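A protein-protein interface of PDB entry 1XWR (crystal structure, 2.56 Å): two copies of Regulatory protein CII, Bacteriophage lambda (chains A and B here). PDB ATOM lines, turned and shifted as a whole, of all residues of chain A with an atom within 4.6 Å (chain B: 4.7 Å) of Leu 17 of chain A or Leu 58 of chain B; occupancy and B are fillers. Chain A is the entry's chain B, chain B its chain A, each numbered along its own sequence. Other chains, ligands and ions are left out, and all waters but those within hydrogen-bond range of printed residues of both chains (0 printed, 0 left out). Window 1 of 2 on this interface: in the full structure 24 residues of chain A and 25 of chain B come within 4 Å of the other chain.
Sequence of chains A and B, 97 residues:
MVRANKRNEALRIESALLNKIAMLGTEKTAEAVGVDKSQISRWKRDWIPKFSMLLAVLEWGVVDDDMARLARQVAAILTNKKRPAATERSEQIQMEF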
ATOM      1  N   ILE A  13      -6.079  -6.935  12.215  1.00  0.00           N
ATOM      2  CA  ILE A  13      -6.171  -7.364  10.836  1.00  0.00           C
ATOM      3  C   ILE A  13      -7.553  -7.924  10.532  1.00  0.00           C
ATOM      4  O   ILE A  13      -8.158  -7.601   9.503  1.00  0.00           O
ATOM      5  CB  ILE A  13      -5.078  -8.406  10.521  1.00  0.00           C
ATOM      6  CG1 ILE A  13      -3.717  -7.709  10.555  1.00  0.00           C
ATOM      7  CG2 ILE A  13      -5.341  -9.090   9.174  1.00  0.00           C
ATOM      8  CD1 ILE A  13      -2.545  -8.646  10.396  1.00  0.00           C
ATOM      9  N   GLU A  14      -8.054  -8.758  11.428  1.00  0.00           N
ATOM     10  CA  GLU A  14      -9.380  -9.342  11.253  1.00  0.00           C
ATOM     11  C   GLU A  14     -10.429  -8.250  11.058  1.00  0.00           C
ATOM     12  O   GLU A  14     -11.265  -8.302  10.153  1.00  0.00           O
ATOM     13  CB  GLU A  14      -9.757 -10.155  12.469  1.00  0.00           C
ATOM     14  CG  GLU A  14     -11.093 -10.826  12.373  1.00  0.00           C
ATOM     15  CD  GLU A  14     -11.436 -11.524  13.667  1.00  0.00           C
ATOM     16  OE1 GLU A  14     -10.487 -11.955  14.363  1.00  0.00           O
ATOM     17  OE2 GLU A  14     -12.637 -11.644  13.989  1.00  0.00           O
ATOM     18  N   SER A  15     -10.364  -7.244  11.906  1.00  0.00           N
ATOM     19  CA  SER A  15     -11.316  -6.159  11.817  1.00  0.00           C
ATOM     20  C   SER A  15     -11.210  -5.477  10.452  1.00  0.00           C
ATOM     21  O   SER A  15     -12.218  -5.214   9.787  1.00  0.00           O
ATOM     22  CB  SER A  15     -11.054  -5.159  12.940  1.00  0.00           C
ATOM     23  OG  SER A  15     -11.869  -4.018  12.779  1.00  0.00           O
ATOM     24  N   ALA A  16      -9.989  -5.190  10.025  1.00  0.00           N
ATOM     25  CA  ALA A  16      -9.825  -4.538   8.736  1.00  0.00           C
ATOM     26  C   ALA A  16     -10.413  -5.426   7.625  1.00  0.00           C
ATOM     27  O   ALA A  16     -11.110  -4.947   6.741  1.00  0.00           O
ATOM     28  CB  ALA A  16      -8.356  -4.247   8.476  1.00  0.00           C
ATOM     29  N   LEU A  17     -10.143  -6.720   7.685  1.00  0.00           N
ATOM     30  CA  LEU A  17     -10.669  -7.632   6.686  1.00  0.00           C
ATOM     31  C   LEU A  17     -12.191  -7.655   6.730  1.00  0.00           C
ATOM     32  O   LEU A  17     -12.862  -7.492   5.702  1.00  0.00           O
ATOM     33  CB  LEU A  17     -10.091  -9.041   6.897  1.00  0.00           C
ATOM     34  CG  LEU A  17      -8.576  -9.099   6.684  1.00  0.00           C
ATOM     35  CD1 LEU A  17      -8.063 -10.487   6.771  1.00  0.00           C
ATOM     36  CD2 LEU A  17      -8.264  -8.545   5.317  1.00  0.00           C
ATOM     37  N   LEU A  18     -12.742  -7.835   7.927  1.00  0.00           N
ATOM     38  CA  LEU A  18     -14.202  -7.851   8.094  1.00  0.00           C
ATOM     39  C   LEU A  18     -14.834  -6.553   7.622  1.00  0.00           C
ATOM     40  O   LEU A  18     -15.894  -6.557   7.013  1.00  0.00           O
ATOM     41  CB  LEU A  18     -14.561  -8.123   9.557  1.00  0.00           C
ATOM     42  CG  LEU A  18     -14.859  -9.565   9.980  1.00  0.00           C
ATOM     43  CD1 LEU A  18     -14.417 -10.567   8.958  1.00  0.00           C
ATOM     44  CD2 LEU A  18     -14.215  -9.842  11.300  1.00  0.00           C
ATOM     45  N   ASN A  19     -14.163  -5.443   7.881  1.00  0.00           N
ATOM     46  CA  ASN A  19     -14.676  -4.146   7.468  1.00  0.00           C
ATOM     47  C   ASN A  19     -14.766  -4.021   5.958  1.00  0.00           C
ATOM     48  O   ASN A  19     -15.791  -3.580   5.424  1.00  0.00           O
ATOM     49  CB  ASN A  19     -13.797  -3.040   8.053  1.00  0.00           C
ATOM     50  CG  ASN A  19     -14.071  -2.818   9.522  1.00  0.00           C
ATOM     51  OD1 ASN A  19     -14.986  -3.433  10.084  1.00  0.00           O
ATOM     52  ND2 ASN A  19     -13.293  -1.940  10.157  1.00  0.00           N
ATOM     53  N   LYS A  20     -13.684  -4.418   5.279  1.00  0.00           N
ATOM     54  CA  LYS A  20     -13.617  -4.371   3.832  1.00  0.00           C
ATOM     55  C   LYS A  20     -14.672  -5.279   3.247  1.00  0.00           C
ATOM     56  O   LYS A  20     -15.425  -4.867   2.378  1.00  0.00           O
ATOM     57  CB  LYS A  20     -12.228  -4.785   3.372  1.00  0.00           C
ATOM     58  CG  LYS A  20     -11.585  -3.752   2.489  1.00  0.00           C
ATOM     59  CD  LYS A  20     -12.374  -3.553   1.198  1.00  0.00           C
ATOM     60  CE  LYS A  20     -11.888  -2.320   0.458  1.00  0.00           C
ATOM     61  NZ  LYS A  20     -10.395  -2.332   0.317  1.00  0.00           N
ATOM     62  N   ILE A  21     -14.741  -6.511   3.735  1.00  0.00           N
ATOM     63  CA  ILE A  21     -15.744  -7.427   3.253  1.00  0.00           C
ATOM     64  C   ILE A  21     -17.121  -6.771   3.383  1.00  0.00           C
ATOM     65  O   ILE A  21     -17.948  -6.875   2.477  1.00  0.00           O
ATOM     66  CB  ILE A  21     -15.711  -8.720   4.045  1.00  0.00           C
ATOM     67  CG1 ILE A  21     -14.439  -9.501   3.679  1.00  0.00           C
ATOM     68  CG2 ILE A  21     -16.989  -9.523   3.786  1.00  0.00           C
ATOM     69  CD1 ILE A  21     -14.173 -10.683   4.545  1.00  0.00           C
ATOM     70  N   LEU A  24     -17.773  -4.148   0.757  1.00  0.00           N
ATOM     71  CA  LEU A  24     -18.003  -4.703  -0.566  1.00  0.00           C
ATOM     72  C   LEU A  24     -19.294  -5.483  -0.567  1.00  0.00           C
ATOM     73  O   LEU A  24     -19.953  -5.595  -1.586  1.00  0.00           O
ATOM     74  CB  LEU A  24     -16.873  -5.656  -0.965  1.00  0.00           C
ATOM     75  CG  LEU A  24     -15.686  -5.210  -1.811  1.00  0.00           C
ATOM     76  CD1 LEU A  24     -14.993  -4.005  -1.213  1.00  0.00           C
ATOM     77  CD2 LEU A  24     -14.734  -6.372  -1.902  1.00  0.00           C
ATOM     78  N   THR A  29     -18.710 -10.482  -1.957  1.00  0.00           N
ATOM     79  CA  THR A  29     -17.365 -10.900  -1.689  1.00  0.00           C
ATOM     80  C   THR A  29     -17.267 -12.412  -1.708  1.00  0.00           C
ATOM     81  O   THR A  29     -16.396 -12.980  -2.372  1.00  0.00           O
ATOM     82  CB  THR A  29     -16.871 -10.340  -0.345  1.00  0.00           C
ATOM     83  OG1 THR A  29     -16.676  -8.923  -0.466  1.00  0.00           O
ATOM     84  CG2 THR A  29     -15.554 -10.983   0.041  1.00  0.00           C
ATOM     85  N   ILE A  48     -11.381 -16.403   8.589  1.00  0.00           N
ATOM     86  CA  ILE A  48     -10.760 -15.092   8.609  1.00  0.00           C
ATOM     87  C   ILE A  48      -9.829 -14.958   9.821  1.00  0.00           C
ATOM     88  O   ILE A  48      -8.669 -14.626   9.695  1.00  0.00           O
ATOM     89  CB  ILE A  48     -11.792 -13.984   8.659  1.00  0.00           C
ATOM     90  CG1 ILE A  48     -12.816 -14.181   7.554  1.00  0.00           C
ATOM     91  CG2 ILE A  48     -11.114 -12.638   8.505  1.00  0.00           C
ATOM     92  CD1 ILE A  48     -12.269 -14.266   6.235  1.00  0.00           C
ATOM     93  N   PHE A  51      -6.571 -16.826   9.183  1.00  0.00           N
ATOM     94  CA  PHE A  51      -5.804 -16.147   8.164  1.00  0.00           C
ATOM     95  C   PHE A  51      -5.222 -14.844   8.732  1.00  0.00           C
ATOM     96  O   PHE A  51      -4.094 -14.467   8.420  1.00  0.00           O
ATOM     97  CB  PHE A  51      -6.709 -15.909   6.956  1.00  0.00           C
ATOM     98  CG  PHE A  51      -6.069 -15.126   5.853  1.00  0.00           C
ATOM     99  CD1 PHE A  51      -4.816 -15.475   5.366  1.00  0.00           C
ATOM    100  CD2 PHE A  51      -6.707 -14.019   5.319  1.00  0.00           C
ATOM    101  CE1 PHE A  51      -4.213 -14.725   4.365  1.00  0.00           C
ATOM    102  CE2 PHE A  51      -6.109 -13.265   4.316  1.00  0.00           C
ATOM    103  CZ  PHE A  51      -4.859 -13.618   3.840  1.00  0.00           C
ATOM    104  N   SER A  52      -5.976 -14.176   9.594  1.00  0.00           N
ATOM    105  CA  SER A  52      -5.514 -12.936  10.204  1.00  0.00           C
ATOM    106  C   SER A  52      -4.295 -13.168  11.061  1.00  0.00           C
ATOM    107  O   SER A  52      -3.425 -12.316  11.146  1.00  0.00           O
ATOM    108  CB  SER A  52      -6.590 -12.330  11.086  1.00  0.00           C
ATOM    109  OG  SER A  52      -7.686 -11.928  10.291  1.00  0.00           O
ATOM    110  N   LEU A  55      -1.380 -13.663   8.806  1.00  0.00           N
ATOM    111  CA  LEU A  55      -0.976 -12.374   8.297  1.00  0.00           C
ATOM    112  C   LEU A  55      -0.220 -11.603   9.359  1.00  0.00           C
ATOM    113  O   LEU A  55       0.660 -10.825   9.049  1.00  0.00           O
ATOM    114  CB  LEU A  55      -2.219 -11.605   7.828  1.00  0.00           C
ATOM    115  CG  LEU A  55      -2.479 -11.453   6.322  1.00  0.00           C
ATOM    116  CD1 LEU A  55      -2.099 -12.700   5.575  1.00  0.00           C
ATOM    117  CD2 LEU A  55      -3.935 -11.116   6.096  1.00  0.00           C
ATOM    118  N   LEU B  54      -9.043 -13.928  -1.601  1.00  0.00           N
ATOM    119  CA  LEU B  54      -9.750 -12.972  -0.768  1.00  0.00           C
ATOM    120  C   LEU B  54      -9.004 -11.649  -0.738  1.00  0.00           C
ATOM    121  O   LEU B  54      -9.608 -10.579  -0.874  1.00  0.00           O
ATOM    122  CB  LEU B  54      -9.873 -13.487   0.659  1.00  0.00           C
ATOM    123  CG  LEU B  54     -10.367 -12.434   1.653  1.00  0.00           C
ATOM    124  CD1 LEU B  54     -11.801 -12.041   1.343  1.00  0.00           C
ATOM    125  CD2 LEU B  54     -10.262 -12.994   3.031  1.00  0.00           C
ATOM    126  N   LEU B  55      -7.697 -11.720  -0.529  1.00  0.00           N
ATOM    127  CA  LEU B  55      -6.872 -10.522  -0.502  1.00  0.00           C
ATOM    128  C   LEU B  55      -6.907  -9.786  -1.839  1.00  0.00           C
ATOM    129  O   LEU B  55      -6.907  -8.558  -1.875  1.00  0.00           O
ATOM    130  CB  LEU B  55      -5.420 -10.866  -0.166  1.00  0.00           C
ATOM    131  CG  LEU B  55      -5.111 -11.009   1.323  1.00  0.00           C
ATOM    132  CD1 LEU B  55      -3.605 -11.061   1.530  1.00  0.00           C
ATOM    133  CD2 LEU B  55      -5.694  -9.803   2.081  1.00  0.00           C
ATOM    134  N   ALA B  56      -6.948 -10.538  -2.935  1.00  0.00           N
ATOM    135  CA  ALA B  56      -6.968  -9.940  -4.273  1.00  0.00           C
ATOM    136  C   ALA B  56      -8.284  -9.216  -4.460  1.00  0.00           C
ATOM    137  O   ALA B  56      -8.327  -8.060  -4.884  1.00  0.00           O
ATOM    138  CB  ALA B  56      -6.779 -11.038  -5.363  1.00  0.00           C
ATOM    139  N   VAL B  57      -9.363  -9.895  -4.130  1.00  0.00           N
ATOM    140  CA  VAL B  57     -10.663  -9.283  -4.249  1.00  0.00           C
ATOM    141  C   VAL B  57     -10.799  -8.069  -3.340  1.00  0.00           C
ATOM    142  O   VAL B  57     -11.358  -7.054  -3.748  1.00  0.00           O
ATOM    143  CB  VAL B  57     -11.774 -10.295  -3.941  1.00  0.00           C
ATOM    144  CG1 VAL B  57     -13.097  -9.601  -3.891  1.00  0.00           C
ATOM    145  CG2 VAL B  57     -11.794 -11.366  -5.027  1.00  0.00           C
ATOM    146  N   LEU B  58     -10.288  -8.150  -2.118  1.00  0.00           N
ATOM    147  CA  LEU B  58     -10.411  -7.008  -1.216  1.00  0.00           C
ATOM    148  C   LEU B  58      -9.591  -5.837  -1.717  1.00  0.00           C
ATOM    149  O   LEU B  58     -10.057  -4.703  -1.684  1.00  0.00           O
ATOM    150  CB  LEU B  58     -10.036  -7.391   0.232  1.00  0.00           C
ATOM    151  CG  LEU B  58     -10.955  -8.448   0.895  1.00  0.00           C
ATOM    152  CD1 LEU B  58     -10.509  -8.706   2.324  1.00  0.00           C
ATOM    153  CD2 LEU B  58     -12.403  -7.991   0.872  1.00  0.00           C
ATOM    154  N   GLU B  59      -8.380  -6.090  -2.207  1.00  0.00           N
ATOM    155  CA  GLU B  59      -7.574  -4.991  -2.736  1.00  0.00           C
ATOM    156  C   GLU B  59      -8.200  -4.381  -3.977  1.00  0.00           C
ATOM    157  O   GLU B  59      -8.116  -3.183  -4.176  1.00  0.00           O
ATOM    158  CB  GLU B  59      -6.162  -5.442  -3.084  1.00  0.00           C
ATOM    159  CG  GLU B  59      -5.130  -4.978  -2.095  1.00  0.00           C
ATOM    160  CD  GLU B  59      -5.009  -3.462  -2.009  1.00  0.00           C
ATOM    161  OE1 GLU B  59      -4.619  -2.984  -0.920  1.00  0.00           O
ATOM    162  OE2 GLU B  59      -5.281  -2.749  -3.010  1.00  0.00           O
ATOM    163  N   TRP B  60      -8.801  -5.209  -4.825  1.00  0.00           N
ATOM    164  CA  TRP B  60      -9.444  -4.717  -6.034  1.00  0.00           C
ATOM    165  C   TRP B  60     -10.377  -3.598  -5.591  1.00  0.00           C
ATOM    166  O   TRP B  60     -10.644  -2.665  -6.332  1.00  0.00           O
ATOM    167  CB  TRP B  60     -10.213  -5.844  -6.705  1.00  0.00           C
ATOM    168  CG  TRP B  60     -10.718  -5.503  -8.057  1.00  0.00           C
ATOM    169  CD1 TRP B  60     -12.001  -5.611  -8.501  1.00  0.00           C
ATOM    170  CD2 TRP B  60      -9.946  -5.040  -9.167  1.00  0.00           C
ATOM    171  NE1 TRP B  60     -12.073  -5.249  -9.818  1.00  0.00           N
ATOM    172  CE2 TRP B  60     -10.826  -4.896 -10.254  1.00  0.00           C
ATOM    173  CE3 TRP B  60      -8.597  -4.732  -9.346  1.00  0.00           C
ATOM    174  CZ2 TRP B  60     -10.403  -4.464 -11.505  1.00  0.00           C
ATOM    175  CZ3 TRP B  60      -8.180  -4.302 -10.581  1.00  0.00           C
ATOM    176  CH2 TRP B  60      -9.078  -4.171 -11.647  1.00  0.00           C
ATOM    177  N   GLY B  61     -10.867  -3.731  -4.364  1.00  0.00           N
ATOM    178  CA  GLY B  61     -11.689  -2.724  -3.710  1.00  0.00           C
ATOM    179  C   GLY B  61     -12.915  -2.085  -4.305  1.00  0.00           C
ATOM    180  O   GLY B  61     -13.634  -2.676  -5.090  1.00  0.00           O
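The backbone carbonyl oxygen (O) of Leu 58 of chain B is in hydrogen-bond range of the side-chain amino group (NZ) of Lys 20 of chain A (3.1 Å).
O of Ile 48 of chain A sits at hydrogen-bond distance from OG of Ser 52 of chain A, at 2.9 Å.
Among the printed residues, merely in contact across the chains: Phe 51 of chain A with Leu 55 of chain B (3.6 Å), Leu 17 of chain A with Leu 58 of chain B (3.7 Å), Ile 21 of chain A with Leu 58 of chain B (3.8 Å), Leu 24 of chain A with Val 57 of chain B (3.9 Å), Leu 24 of chain A with Leu 58 of chain B (3.97 Å) and Ile 48 of chain A with Leu 54 of chain B (3.99 Å).
Leu 17 of chain A touches just one residue of chain B: Leu 58 (3.7 Å). Of chain A, only Leu 17 (3.7 Å), Lys 20 (3.1 Å), Ile 21 (3.8 Å) and Leu 24 (3.97 Å) come within 4 Å of Leu 58 of chain B. Of the printed residues of chain B, Lys 20 of chain A touches Leu 58 (3.1 Å). Of the printed residues of chain B, Phe 51 of chain A touches Leu 55. Of the printed residues of chain A, Leu 55 of chain B touches Phe 51. Leu 55 of chain A touches none of the printed residues of chain B. The nearest residue of chain A that does not touch Leu 58 of chain B is Thr 29 of chain A (4.4 Å). The nearest printed residue of chain A that does not touch Leu 55 of chain B is Leu 17 of chain A (4.3 Å).
Printed residues of chain A that touch a printed residue of chain B: Leu 17, Lys 20, Ile 21, Leu 24, Ile 48 and Phe 51. Hydrophobic or aromatic side chains of chain A within 4 Å of the printed part of chain B: Leu 17, Ile 21, Leu 24, Ile 48 and Phe 51. Among the printed residues, no Asp or Glu carboxylate lies within 4 Å of a Lys or Arg side-chain nitrogen of the other chain.
Position printed for both chains: 55.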
